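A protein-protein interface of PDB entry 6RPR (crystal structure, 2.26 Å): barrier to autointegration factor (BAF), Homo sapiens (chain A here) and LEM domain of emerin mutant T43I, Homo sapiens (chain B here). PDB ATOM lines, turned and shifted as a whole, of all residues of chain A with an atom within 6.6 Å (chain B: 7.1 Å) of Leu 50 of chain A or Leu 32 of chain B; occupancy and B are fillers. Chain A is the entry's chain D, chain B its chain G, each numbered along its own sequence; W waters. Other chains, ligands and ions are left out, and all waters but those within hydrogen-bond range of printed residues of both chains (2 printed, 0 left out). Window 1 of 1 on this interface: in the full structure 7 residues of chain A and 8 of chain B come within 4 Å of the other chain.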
ATOM      1  N   GLY A  45      23.522  -1.826 -24.168  1.00  0.00           N
ATOM      2  CA  GLY A  45      23.531  -0.487 -24.761  1.00  0.00           C
ATOM      3  C   GLY A  45      23.631   0.609 -23.721  1.00  0.00           C
ATOM      4  O   GLY A  45      24.407   1.549 -23.885  1.00  0.00           O
ATOM      5  N   GLN A  46      22.876   0.462 -22.614  1.00  0.00           N
ATOM      6  CA  GLN A  46      22.888   1.368 -21.463  1.00  0.00           C
ATOM      7  C   GLN A  46      24.259   1.372 -20.775  1.00  0.00           C
ATOM      8  O   GLN A  46      24.803   2.432 -20.467  1.00  0.00           O
ATOM      9  CB  GLN A  46      21.777   0.995 -20.470  1.00  0.00           C
ATOM     10  CG  GLN A  46      21.622   1.990 -19.321  1.00  0.00           C
ATOM     11  CD  GLN A  46      21.141   3.359 -19.719  1.00  0.00           C
ATOM     12  OE1 GLN A  46      20.745   3.620 -20.864  1.00  0.00           O
ATOM     13  NE2 GLN A  46      21.170   4.273 -18.771  1.00  0.00           N
ATOM     14  N   PHE A  47      24.807   0.173 -20.549  1.00  0.00           N
ATOM     15  CA  PHE A  47      26.125  -0.063 -19.983  1.00  0.00           C
ATOM     16  C   PHE A  47      27.221   0.640 -20.828  1.00  0.00           C
ATOM     17  O   PHE A  47      28.137   1.217 -20.260  1.00  0.00           O
ATOM     18  CB  PHE A  47      26.349  -1.588 -19.891  1.00  0.00           C
ATOM     19  CG  PHE A  47      27.752  -2.087 -19.647  1.00  0.00           C
ATOM     20  CD1 PHE A  47      28.260  -2.176 -18.356  1.00  0.00           C
ATOM     21  CD2 PHE A  47      28.539  -2.536 -20.699  1.00  0.00           C
ATOM     22  CE1 PHE A  47      29.532  -2.693 -18.127  1.00  0.00           C
ATOM     23  CE2 PHE A  47      29.803  -3.066 -20.465  1.00  0.00           C
ATOM     24  CZ  PHE A  47      30.292  -3.132 -19.185  1.00  0.00           C
ATOM     25  N   LEU A  48      27.066   0.645 -22.164  1.00  0.00           N
ATOM     26  CA  LEU A  48      27.988   1.279 -23.116  1.00  0.00           C
ATOM     27  C   LEU A  48      27.890   2.811 -23.158  1.00  0.00           C
ATOM     28  O   LEU A  48      28.945   3.469 -23.181  1.00  0.00           O
ATOM     29  CB  LEU A  48      27.850   0.684 -24.531  1.00  0.00           C
ATOM     30  CG  LEU A  48      28.164  -0.824 -24.711  1.00  0.00           C
ATOM     31  CD1 LEU A  48      27.816  -1.304 -26.149  1.00  0.00           C
ATOM     32  CD2 LEU A  48      29.600  -1.163 -24.319  1.00  0.00           C
ATOM     33  N   VAL A  49      26.645   3.390 -23.166  1.00  0.00           N
ATOM     34  CA  VAL A  49      26.484   4.854 -23.127  1.00  0.00           C
ATOM     35  C   VAL A  49      26.965   5.410 -21.788  1.00  0.00           C
ATOM     36  O   VAL A  49      27.366   6.574 -21.740  1.00  0.00           O
ATOM     37  CB  VAL A  49      25.098   5.450 -23.533  1.00  0.00           C
ATOM     38  CG1 VAL A  49      24.853   5.297 -25.017  1.00  0.00           C
ATOM     39  CG2 VAL A  49      23.936   4.898 -22.695  1.00  0.00           C
ATOM     40  N   LEU A  50      26.975   4.566 -20.714  1.00  0.00           N
ATOM     41  CA  LEU A  50      27.507   4.935 -19.399  1.00  0.00           C
ATOM     42  C   LEU A  50      29.027   4.676 -19.293  1.00  0.00           C
ATOM     43  O   LEU A  50      29.587   4.761 -18.196  1.00  0.00           O
ATOM     44  CB  LEU A  50      26.746   4.271 -18.238  1.00  0.00           C
ATOM     45  CG  LEU A  50      25.281   4.697 -18.043  1.00  0.00           C
ATOM     46  CD1 LEU A  50      24.590   3.747 -17.099  1.00  0.00           C
ATOM     47  CD2 LEU A  50      25.171   6.142 -17.536  1.00  0.00           C
ATOM     48  N   LYS A  51      29.681   4.386 -20.442  1.00  0.00           N
ATOM     49  CA  LYS A  51      31.106   4.130 -20.620  1.00  0.00           C
ATOM     50  C   LYS A  51      31.615   2.947 -19.787  1.00  0.00           C
ATOM     51  O   LYS A  51      32.774   2.942 -19.360  1.00  0.00           O
ATOM     52  CB  LYS A  51      31.927   5.412 -20.384  1.00  0.00           C
ATOM     53  CG  LYS A  51      31.851   6.384 -21.571  1.00  0.00           C
ATOM     54  CD  LYS A  51      32.610   7.658 -21.278  1.00  0.00           C
ATOM     55  CE  LYS A  51      32.899   8.426 -22.539  1.00  0.00           C
ATOM     56  NZ  LYS A  51      33.377   9.812 -22.265  1.00  0.00           N
ATOM     57  N   LYS A  52      30.751   1.911 -19.603  1.00  0.00           N
ATOM     58  CA  LYS A  52      31.035   0.678 -18.844  1.00  0.00           C
ATOM     59  C   LYS A  52      31.321   0.983 -17.359  1.00  0.00           C
ATOM     60  O   LYS A  52      31.970   0.185 -16.683  1.00  0.00           O
ATOM     61  CB  LYS A  52      32.203  -0.104 -19.478  1.00  0.00           C
ATOM     62  CG  LYS A  52      32.062  -0.381 -20.973  1.00  0.00           C
ATOM     63  CD  LYS A  52      33.354  -0.936 -21.506  1.00  0.00           C
ATOM     64  CE  LYS A  52      33.224  -1.356 -22.953  1.00  0.00           C
ATOM     65  NZ  LYS A  52      34.552  -1.520 -23.600  1.00  0.00           N
ATOM     66  N   ASP A  53      30.842   2.137 -16.863  1.00  0.00           N
ATOM     67  CA  ASP A  53      31.053   2.588 -15.485  1.00  0.00           C
ATOM     68  C   ASP A  53      30.192   1.820 -14.478  1.00  0.00           C
ATOM     69  O   ASP A  53      28.962   1.795 -14.618  1.00  0.00           O
ATOM     70  CB  ASP A  53      30.802   4.100 -15.368  1.00  0.00           C
ATOM     71  CG  ASP A  53      31.210   4.677 -14.035  1.00  0.00           C
ATOM     72  OD1 ASP A  53      32.415   4.976 -13.863  1.00  0.00           O
ATOM     73  OD2 ASP A  53      30.337   4.805 -13.153  1.00  0.00           O
ATOM     74  N   GLU A  54      30.849   1.216 -13.449  1.00  0.00           N
ATOM     75  CA  GLU A  54      30.195   0.442 -12.394  1.00  0.00           C
ATOM     76  C   GLU A  54      29.212   1.257 -11.572  1.00  0.00           C
ATOM     77  O   GLU A  54      28.059   0.858 -11.458  1.00  0.00           O
ATOM     78  CB  GLU A  54      31.208  -0.278 -11.484  1.00  0.00           C
ATOM     79  CG  GLU A  54      30.549  -1.305 -10.570  1.00  0.00           C
ATOM     80  CD  GLU A  54      31.443  -2.296  -9.851  1.00  0.00           C
ATOM     81  OE1 GLU A  54      30.902  -3.082  -9.039  1.00  0.00           O
ATOM     82  OE2 GLU A  54      32.669  -2.312 -10.109  1.00  0.00           O
ATOM     83  N   ASP A  55      29.661   2.390 -11.011  1.00  0.00           N
ATOM     84  CA  ASP A  55      28.813   3.237 -10.174  1.00  0.00           C
ATOM     85  C   ASP A  55      27.587   3.731 -10.897  1.00  0.00           C
ATOM     86  O   ASP A  55      26.483   3.586 -10.373  1.00  0.00           O
ATOM     87  CB  ASP A  55      29.609   4.399  -9.563  1.00  0.00           C
ATOM     88  CG  ASP A  55      30.565   3.972  -8.462  1.00  0.00           C
ATOM     89  OD1 ASP A  55      30.231   3.007  -7.719  1.00  0.00           O
ATOM     90  OD2 ASP A  55      31.645   4.610  -8.329  1.00  0.00           O
ATOM     91  N   LEU A  56      27.777   4.266 -12.121  1.00  0.00           N
ATOM     92  CA  LEU A  56      26.698   4.796 -12.951  1.00  0.00           C
ATOM     93  C   LEU A  56      25.682   3.762 -13.382  1.00  0.00           C
ATOM     94  O   LEU A  56      24.486   4.052 -13.335  1.00  0.00           O
ATOM     95  CB  LEU A  56      27.244   5.563 -14.165  1.00  0.00           C
ATOM     96  CG  LEU A  56      27.777   6.965 -13.851  1.00  0.00           C
ATOM     97  CD1 LEU A  56      28.312   7.638 -15.102  1.00  0.00           C
ATOM     98  CD2 LEU A  56      26.709   7.824 -13.159  1.00  0.00           C
ATOM     99  N   PHE A  57      26.132   2.568 -13.785  1.00  0.00           N
ATOM    100  CA  PHE A  57      25.248   1.491 -14.227  1.00  0.00           C
ATOM    101  C   PHE A  57      24.423   0.905 -13.083  1.00  0.00           C
ATOM    102  O   PHE A  57      23.211   0.717 -13.227  1.00  0.00           O
ATOM    103  CB  PHE A  57      26.032   0.396 -14.974  1.00  0.00           C
ATOM    104  CG  PHE A  57      25.183  -0.759 -15.448  1.00  0.00           C
ATOM    105  CD1 PHE A  57      24.439  -0.663 -16.622  1.00  0.00           C
ATOM    106  CD2 PHE A  57      25.087  -1.926 -14.694  1.00  0.00           C
ATOM    107  CE1 PHE A  57      23.636  -1.727 -17.047  1.00  0.00           C
ATOM    108  CE2 PHE A  57      24.269  -2.981 -15.110  1.00  0.00           C
ATOM    109  CZ  PHE A  57      23.551  -2.871 -16.284  1.00  0.00           C
ATOM    110  N   ARG A  58      25.090   0.582 -11.963  1.00  0.00           N
ATOM    111  CA  ARG A  58      24.427   0.014 -10.786  1.00  0.00           C
ATOM    112  C   ARG A  58      23.381   0.976 -10.202  1.00  0.00           C
ATOM    113  O   ARG A  58      22.281   0.546  -9.840  1.00  0.00           O
ATOM    114  CB  ARG A  58      25.459  -0.439  -9.762  1.00  0.00           C
ATOM    115  CG  ARG A  58      26.244  -1.639 -10.274  1.00  0.00           C
ATOM    116  CD  ARG A  58      27.155  -2.231  -9.234  1.00  0.00           C
ATOM    117  NE  ARG A  58      26.412  -2.674  -8.056  1.00  0.00           N
ATOM    118  CZ  ARG A  58      26.975  -3.193  -6.971  1.00  0.00           C
ATOM    119  NH1 ARG A  58      28.289  -3.359  -6.912  1.00  0.00           N
ATOM    120  NH2 ARG A  58      26.227  -3.554  -5.940  1.00  0.00           N
ATOM    121  N   GLU A  59      23.697   2.279 -10.197  1.00  0.00           N
ATOM    122  CA  GLU A  59      22.798   3.331  -9.722  1.00  0.00           C
ATOM    123  C   GLU A  59      21.576   3.474 -10.640  1.00  0.00           C
ATOM    124  O   GLU A  59      20.462   3.577 -10.138  1.00  0.00           O
ATOM    125  CB  GLU A  59      23.552   4.658  -9.584  1.00  0.00           C
ATOM    126  CG  GLU A  59      22.898   5.646  -8.639  1.00  0.00           C
ATOM    127  CD  GLU A  59      23.526   7.025  -8.604  1.00  0.00           C
ATOM    128  OE1 GLU A  59      22.779   8.000  -8.359  1.00  0.00           O
ATOM    129  OE2 GLU A  59      24.759   7.136  -8.811  1.00  0.00           O
ATOM    130  N   TRP A  60      21.787   3.463 -11.979  1.00  0.00           N
ATOM    131  CA  TRP A  60      20.714   3.513 -12.983  1.00  0.00           C
ATOM    132  C   TRP A  60      19.776   2.306 -12.811  1.00  0.00           C
ATOM    133  O   TRP A  60      18.565   2.491 -12.815  1.00  0.00           O
ATOM    134  CB  TRP A  60      21.279   3.571 -14.437  1.00  0.00           C
ATOM    135  CG  TRP A  60      20.236   3.326 -15.488  1.00  0.00           C
ATOM    136  CD1 TRP A  60      19.257   4.194 -15.889  1.00  0.00           C
ATOM    137  CD2 TRP A  60      19.946   2.074 -16.124  1.00  0.00           C
ATOM    138  NE1 TRP A  60      18.403   3.569 -16.775  1.00  0.00           N
ATOM    139  CE2 TRP A  60      18.807   2.268 -16.939  1.00  0.00           C
ATOM    140  CE3 TRP A  60      20.551   0.804 -16.096  1.00  0.00           C
ATOM    141  CZ2 TRP A  60      18.264   1.245 -17.719  1.00  0.00           C
ATOM    142  CZ3 TRP A  60      20.023  -0.204 -16.881  1.00  0.00           C
ATOM    143  CH2 TRP A  60      18.895   0.021 -17.686  1.00  0.00           C
ATOM    144  N   ASP A  63      17.658   2.676  -9.642  1.00  0.00           N
ATOM    145  CA  ASP A  63      16.677   3.736  -9.868  1.00  0.00           C
ATOM    146  C   ASP A  63      15.575   3.395 -10.874  1.00  0.00           C
ATOM    147  O   ASP A  63      14.441   3.863 -10.718  1.00  0.00           O
ATOM    148  CB  ASP A  63      17.382   5.042 -10.298  1.00  0.00           C
ATOM    149  CG  ASP A  63      18.305   5.697  -9.276  1.00  0.00           C
ATOM    150  OD1 ASP A  63      18.249   5.313  -8.080  1.00  0.00           O
ATOM    151  OD2 ASP A  63      19.088   6.590  -9.673  1.00  0.00           O
ATOM    152  N   LEU B  11      23.703  20.811 -19.935  1.00  0.00           N
ATOM    153  CA  LEU B  11      23.738  19.857 -18.822  1.00  0.00           C
ATOM    154  C   LEU B  11      25.131  19.230 -18.718  1.00  0.00           C
ATOM    155  O   LEU B  11      25.635  19.049 -17.610  1.00  0.00           O
ATOM    156  CB  LEU B  11      22.645  18.774 -18.980  1.00  0.00           C
ATOM    157  CG  LEU B  11      22.149  18.116 -17.674  1.00  0.00           C
ATOM    158  CD1 LEU B  11      21.105  18.980 -16.959  1.00  0.00           C
ATOM    159  CD2 LEU B  11      21.619  16.706 -17.921  1.00  0.00           C
ATOM    160  N   LEU B  15      28.048  19.287 -15.942  1.00  0.00           N
ATOM    161  CA  LEU B  15      28.633  18.046 -15.400  1.00  0.00           C
ATOM    162  C   LEU B  15      30.152  18.205 -15.326  1.00  0.00           C
ATOM    163  O   LEU B  15      30.771  17.756 -14.369  1.00  0.00           O
ATOM    164  CB  LEU B  15      28.308  16.814 -16.279  1.00  0.00           C
ATOM    165  CG  LEU B  15      26.869  16.284 -16.309  1.00  0.00           C
ATOM    166  CD1 LEU B  15      26.675  15.384 -17.502  1.00  0.00           C
ATOM    167  CD2 LEU B  15      26.492  15.584 -14.997  1.00  0.00           C
ATOM    168  N   HIS B  22      30.975  11.361 -15.850  1.00  0.00           N
ATOM    169  CA  HIS B  22      29.874  11.174 -16.770  1.00  0.00           C
ATOM    170  C   HIS B  22      30.271  10.667 -18.152  1.00  0.00           C
ATOM    171  O   HIS B  22      31.413  10.770 -18.580  1.00  0.00           O
ATOM    172  CB  HIS B  22      29.114  12.530 -16.913  1.00  0.00           C
ATOM    173  CG  HIS B  22      29.892  13.570 -17.661  1.00  0.00           C
ATOM    174  ND1 HIS B  22      30.966  14.217 -17.086  1.00  0.00           N
ATOM    175  CD2 HIS B  22      29.770  13.983 -18.942  1.00  0.00           C
ATOM    176  CE1 HIS B  22      31.442  15.020 -18.021  1.00  0.00           C
ATOM    177  NE2 HIS B  22      30.755  14.911 -19.153  1.00  0.00           N
ATOM    178  N   GLY B  23      29.271  10.168 -18.847  1.00  0.00           N
ATOM    179  CA  GLY B  23      29.347   9.774 -20.240  1.00  0.00           C
ATOM    180  C   GLY B  23      28.445  10.757 -20.953  1.00  0.00           C
ATOM    181  O   GLY B  23      27.983  11.723 -20.321  1.00  0.00           O
ATOM    182  N   PRO B  24      28.110  10.523 -22.239  1.00  0.00           N
ATOM    183  CA  PRO B  24      27.184  11.430 -22.928  1.00  0.00           C
ATOM    184  C   PRO B  24      25.772  11.545 -22.327  1.00  0.00           C
ATOM    185  O   PRO B  24      25.281  10.631 -21.660  1.00  0.00           O
ATOM    186  CB  PRO B  24      27.112  10.837 -24.332  1.00  0.00           C
ATOM    187  CG  PRO B  24      27.542   9.437 -24.188  1.00  0.00           C
ATOM    188  CD  PRO B  24      28.574   9.456 -23.144  1.00  0.00           C
ATOM    189  N   GLY B  27      18.701  10.427 -24.070  1.00  0.00           N
ATOM    190  CA  GLY B  27      17.385  10.167 -23.476  1.00  0.00           C
ATOM    191  C   GLY B  27      17.384   9.235 -22.271  1.00  0.00           C
ATOM    192  O   GLY B  27      16.774   9.551 -21.241  1.00  0.00           O
ATOM    193  N   SER B  28      18.116   8.099 -22.358  1.00  0.00           N
ATOM    194  CA  SER B  28      18.194   7.091 -21.285  1.00  0.00           C
ATOM    195  C   SER B  28      19.151   7.431 -20.130  1.00  0.00           C
ATOM    196  O   SER B  28      19.198   6.672 -19.157  1.00  0.00           O
ATOM    197  CB  SER B  28      18.538   5.722 -21.864  1.00  0.00           C
ATOM    198  OG  SER B  28      19.851   5.683 -22.400  1.00  0.00           O
ATOM    199  N   THR B  29      19.914   8.553 -20.231  1.00  0.00           N
ATOM    200  CA  THR B  29      20.879   8.984 -19.204  1.00  0.00           C
ATOM    201  C   THR B  29      20.541  10.351 -18.555  1.00  0.00           C
ATOM    202  O   THR B  29      21.063  10.676 -17.477  1.00  0.00           O
ATOM    203  CB  THR B  29      22.327   8.976 -19.749  1.00  0.00           C
ATOM    204  OG1 THR B  29      22.480   9.999 -20.736  1.00  0.00           O
ATOM    205  CG2 THR B  29      22.766   7.610 -20.284  1.00  0.00           C
ATOM    206  N   ARG B  30      19.695  11.147 -19.232  1.00  0.00           N
ATOM    207  CA  ARG B  30      19.270  12.497 -18.833  1.00  0.00           C
ATOM    208  C   ARG B  30      18.865  12.613 -17.350  1.00  0.00           C
ATOM    209  O   ARG B  30      19.454  13.421 -16.631  1.00  0.00           O
ATOM    210  CB  ARG B  30      18.147  12.993 -19.776  1.00  0.00           C
ATOM    211  CG  ARG B  30      17.571  14.377 -19.445  1.00  0.00           C
ATOM    212  CD  ARG B  30      18.439  15.528 -19.914  1.00  0.00           C
ATOM    213  NE  ARG B  30      18.077  16.755 -19.210  1.00  0.00           N
ATOM    214  CZ  ARG B  30      18.121  17.974 -19.740  1.00  0.00           C
ATOM    215  NH1 ARG B  30      18.517  18.147 -20.995  1.00  0.00           N
ATOM    216  NH2 ARG B  30      17.760  19.027 -19.023  1.00  0.00           N
ATOM    217  N   ARG B  31      17.865  11.812 -16.913  1.00  0.00           N
ATOM    218  CA  ARG B  31      17.344  11.774 -15.547  1.00  0.00           C
ATOM    219  C   ARG B  31      18.438  11.480 -14.507  1.00  0.00           C
ATOM    220  O   ARG B  31      18.479  12.120 -13.446  1.00  0.00           O
ATOM    221  CB  ARG B  31      16.171  10.770 -15.416  1.00  0.00           C
ATOM    222  CG  ARG B  31      15.299  11.025 -14.172  1.00  0.00           C
ATOM    223  CD  ARG B  31      14.258   9.948 -13.863  1.00  0.00           C
ATOM    224  NE  ARG B  31      13.154   9.910 -14.831  1.00  0.00           N
ATOM    225  CZ  ARG B  31      12.088  10.708 -14.808  1.00  0.00           C
ATOM    226  NH1 ARG B  31      11.962  11.637 -13.866  1.00  0.00           N
ATOM    227  NH2 ARG B  31      11.147  10.593 -15.735  1.00  0.00           N
ATOM    228  N   LEU B  32      19.307  10.511 -14.809  1.00  0.00           N
ATOM    229  CA  LEU B  32      20.404  10.139 -13.924  1.00  0.00           C
ATOM    230  C   LEU B  32      21.393  11.304 -13.703  1.00  0.00           C
ATOM    231  O   LEU B  32      21.797  11.534 -12.563  1.00  0.00           O
ATOM    232  CB  LEU B  32      21.111   8.872 -14.445  1.00  0.00           C
ATOM    233  CG  LEU B  32      22.334   8.387 -13.651  1.00  0.00           C
ATOM    234  CD1 LEU B  32      21.921   7.551 -12.419  1.00  0.00           C
ATOM    235  CD2 LEU B  32      23.282   7.634 -14.542  1.00  0.00           C
ATOM    236  N   TYR B  33      21.736  12.060 -14.765  1.00  0.00           N
ATOM    237  CA  TYR B  33      22.686  13.168 -14.652  1.00  0.00           C
ATOM    238  C   TYR B  33      22.072  14.374 -13.975  1.00  0.00           C
ATOM    239  O   TYR B  33      22.763  15.036 -13.197  1.00  0.00           O
ATOM    240  CB  TYR B  33      23.358  13.510 -15.987  1.00  0.00           C
ATOM    241  CG  TYR B  33      24.278  12.405 -16.461  1.00  0.00           C
ATOM    242  CD1 TYR B  33      25.248  11.863 -15.614  1.00  0.00           C
ATOM    243  CD2 TYR B  33      24.207  11.921 -17.767  1.00  0.00           C
ATOM    244  CE1 TYR B  33      26.090  10.836 -16.041  1.00  0.00           C
ATOM    245  CE2 TYR B  33      25.056  10.906 -18.208  1.00  0.00           C
ATOM    246  CZ  TYR B  33      25.997  10.370 -17.342  1.00  0.00           C
ATOM    247  OH  TYR B  33      26.837   9.374 -17.774  1.00  0.00           O
ATOM    248  N   GLU B  34      20.769  14.610 -14.204  1.00  0.00           N
ATOM    249  CA  GLU B  34      19.980  15.648 -13.528  1.00  0.00           C
ATOM    250  C   GLU B  34      19.980  15.391 -11.996  1.00  0.00           C
ATOM    251  O   GLU B  34      20.116  16.340 -11.232  1.00  0.00           O
ATOM    252  CB  GLU B  34      18.540  15.648 -14.060  1.00  0.00           C
ATOM    253  CG  GLU B  34      18.332  16.556 -15.255  1.00  0.00           C
ATOM    254  CD  GLU B  34      16.876  16.875 -15.525  1.00  0.00           C
ATOM    255  OE1 GLU B  34      16.503  16.960 -16.716  1.00  0.00           O
ATOM    256  OE2 GLU B  34      16.106  17.038 -14.550  1.00  0.00           O
ATOM    257  N   LYS B  35      19.876  14.100 -11.575  1.00  0.00           N
ATOM    258  CA  LYS B  35      19.909  13.640 -10.179  1.00  0.00           C
ATOM    259  C   LYS B  35      21.305  13.874  -9.582  1.00  0.00           C
ATOM    260  O   LYS B  35      21.415  14.295  -8.425  1.00  0.00           O
ATOM    261  CB  LYS B  35      19.527  12.146 -10.100  1.00  0.00           C
ATOM    262  CG  LYS B  35      19.516  11.552  -8.700  1.00  0.00           C
ATOM    263  CD  LYS B  35      19.841  10.076  -8.746  1.00  0.00           C
ATOM    264  CE  LYS B  35      19.641   9.390  -7.417  1.00  0.00           C
ATOM    265  NZ  LYS B  35      20.106   7.975  -7.457  1.00  0.00           N
ATOM    266  N   LYS B  36      22.366  13.591 -10.372  1.00  0.00           N
ATOM    267  CA  LYS B  36      23.752  13.812  -9.949  1.00  0.00           C
ATOM    268  C   LYS B  36      24.061  15.320  -9.803  1.00  0.00           C
ATOM    269  O   LYS B  36      24.733  15.696  -8.845  1.00  0.00           O
ATOM    270  CB  LYS B  36      24.750  13.074 -10.864  1.00  0.00           C
ATOM    271  CG  LYS B  36      24.609  11.547 -10.799  1.00  0.00           C
ATOM    272  CD  LYS B  36      25.860  10.820 -10.305  1.00  0.00           C
ATOM    273  CE  LYS B  36      26.045  10.810  -8.795  1.00  0.00           C
ATOM    274  NZ  LYS B  36      25.175   9.826  -8.099  1.00  0.00           N
ATOM    275  N   ILE B  37      23.515  16.177 -10.706  1.00  0.00           N
ATOM    276  CA  ILE B  37      23.659  17.639 -10.654  1.00  0.00           C
ATOM    277  C   ILE B  37      22.937  18.183  -9.406  1.00  0.00           C
ATOM    278  O   ILE B  37      23.508  19.021  -8.692  1.00  0.00           O
ATOM    279  CB  ILE B  37      23.263  18.356 -11.996  1.00  0.00           C
ATOM    280  CG1 ILE B  37      24.251  17.971 -13.108  1.00  0.00           C
ATOM    281  CG2 ILE B  37      23.240  19.895 -11.841  1.00  0.00           C
ATOM    282  CD1 ILE B  37      23.891  18.383 -14.491  1.00  0.00           C
ATOM    283  N   PHE B  38      21.728  17.639  -9.110  1.00  0.00           N
ATOM    284  CA  PHE B  38      20.934  17.963  -7.924  1.00  0.00           C
ATOM    285  C   PHE B  38      21.658  17.563  -6.651  1.00  0.00           C
ATOM    286  O   PHE B  38      21.737  18.387  -5.745  1.00  0.00           O
ATOM    287  CB  PHE B  38      19.509  17.338  -7.969  1.00  0.00           C
ATOM    288  CG  PHE B  38      18.663  17.671  -6.751  1.00  0.00           C
ATOM    289  CD1 PHE B  38      17.865  18.810  -6.728  1.00  0.00           C
ATOM    290  CD2 PHE B  38      18.704  16.871  -5.610  1.00  0.00           C
ATOM    291  CE1 PHE B  38      17.104  19.127  -5.601  1.00  0.00           C
ATOM    292  CE2 PHE B  38      17.947  17.193  -4.478  1.00  0.00           C
ATOM    293  CZ  PHE B  38      17.156  18.320  -4.482  1.00  0.00           C
ATOM    294  N   GLU B  39      22.169  16.306  -6.563  1.00  0.00           N
ATOM    295  CA  GLU B  39      22.915  15.816  -5.390  1.00  0.00           C
ATOM    296  C   GLU B  39      24.143  16.704  -5.125  1.00  0.00           C
ATOM    297  O   GLU B  39      24.458  16.973  -3.964  1.00  0.00           O
ATOM    298  CB  GLU B  39      23.398  14.359  -5.576  1.00  0.00           C
ATOM    299  CG  GLU B  39      22.312  13.299  -5.504  1.00  0.00           C
ATOM    300  CD  GLU B  39      22.711  11.877  -5.872  1.00  0.00           C
ATOM    301  OE1 GLU B  39      23.776  11.684  -6.501  1.00  0.00           O
ATOM    302  OE2 GLU B  39      21.943  10.948  -5.533  1.00  0.00           O
HETATM  303  O   HOH W   1      31.722  11.947 -21.272  1.00  0.00           O
HETATM  304  O   HOH W   2      26.242   8.447 -20.204  1.00  0.00           O
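The side-chain amide oxygen of Gln 46 of chain A lies within hydrogen-bond range of the side-chain hydroxyl of Ser 28 of chain B, at 2.7 Å. The side-chain carboxylate (OD2) of Asp 63 of chain A lies within salt-bridge range of the side-chain amino group (NZ) of Lys 35 of chain B, at 2.8 Å. NZ of Lys 36 of chain B is in salt-bridge range of OE2 of Glu 59 of chain A (2.8 Å). The side-chain carboxylate (OE1) of Glu 59 of chain A lies within salt-bridge range of the side-chain amino group (NZ) of Lys 35 of chain B, 2.8 Å away.
The side-chain amino group of Lys 35 of chain B lies within salt-bridge range of the side-chain carboxylate of Glu 39 of chain B (3.99 Å). The side-chain carboxylate (OD2) of Asp 53 of chain A is in hydrogen-bond range of the backbone NH (N) of Leu 56 of chain A, 2.8 Å away. N of Gly 23 of chain B lies within hydrogen-bond range of OH of Tyr 33 of chain B (2.8 Å). The side-chain hydroxyl (OG1) of Thr 29 of chain B is in hydrogen-bond range of the backbone carbonyl oxygen (O) of Pro 24 of chain B (3.0 Å). The side-chain carboxylate (OE1) of Glu 39 of chain B lies within salt-bridge range of the side-chain amino group (NZ) of Lys 36 of chain B (2.8 Å). The side-chain amide nitrogen (NE2) of Gln 46 of chain A sits close to the indole nitrogen (NE1) of Trp 60 of chain A (3.5 Å).
Among the printed residues, pairs that only touch across the chains: Val 49 of chain A with Pro 24 of chain B (3.4 Å), Leu 56 of chain A with Tyr 33 of chain B (3.5 Å), Leu 50 of chain A with Tyr 33 of chain B (3.6 Å), Leu 56 of chain A with Leu 32 of chain B (3.7 Å), Val 49 of chain A with Thr 29 of chain B (3.8 Å), Leu 50 of chain A with Leu 32 of chain B (3.8 Å), Leu 50 of chain A with Thr 29 of chain B (3.9 Å), Trp 60 of chain A with Ser 28 of chain B (3.99 Å) and Gln 46 of chain A with Thr 29 of chain B (3.996 Å).
Leu 48 of chain A touches none of the printed residues of chain B. Leu 50 of chain A touches just these residues of chain B: Thr 29 (3.9 Å), Leu 32 (3.8 Å) and Tyr 33 (3.6 Å). Of the printed residues of chain B, Trp 60 of chain A touches Ser 28. Of the printed residues of chain A, Thr 29 of chain B touches Gln 46, Val 49 and Leu 50. Leu 32 of chain B touches just these residues of chain A: Leu 50 and Leu 56. The nearest residue of chain B that does not touch Leu 50 of chain A is Gly 23 of chain B (5.2 Å). The nearest printed residue of chain B that does not touch Val 49 of chain A is Gly 23 of chain B (4.1 Å).
Of the 18 printed residues of chain B, 7 touch a printed residue of chain A. Of the 17 printed residues of chain A, 7 touch a printed residue of chain B. Hydrophobic or aromatic side chains of chain A that line the printed part of chain B: Val 49, Leu 50, Leu 56 and Trp 60. Among the printed residues, 13 pairs touch across the chains. Among the printed residues, Asp or Glu carboxylates within 4 Å of a Lys or Arg side-chain nitrogen of the other chain: Glu 59 of chain A with Lys 35 of chain B (2.8 Å), Glu 59 of chain A with Lys 36 of chain B (2.8 Å) and Asp 63 of chain A with Lys 35 of chain B (2.8 Å).
Water W2 lies within hydrogen-bond range of OH of Tyr 33 of chain B, O of Val 49 of chain A and O of Pro 24 of chain B. Water W1 lies within hydrogen-bond range of the side-chain amino group of Lys 51 of chain A (2.9 Å) and the backbone carbonyl oxygen of His 22 of chain B (3.0 Å).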
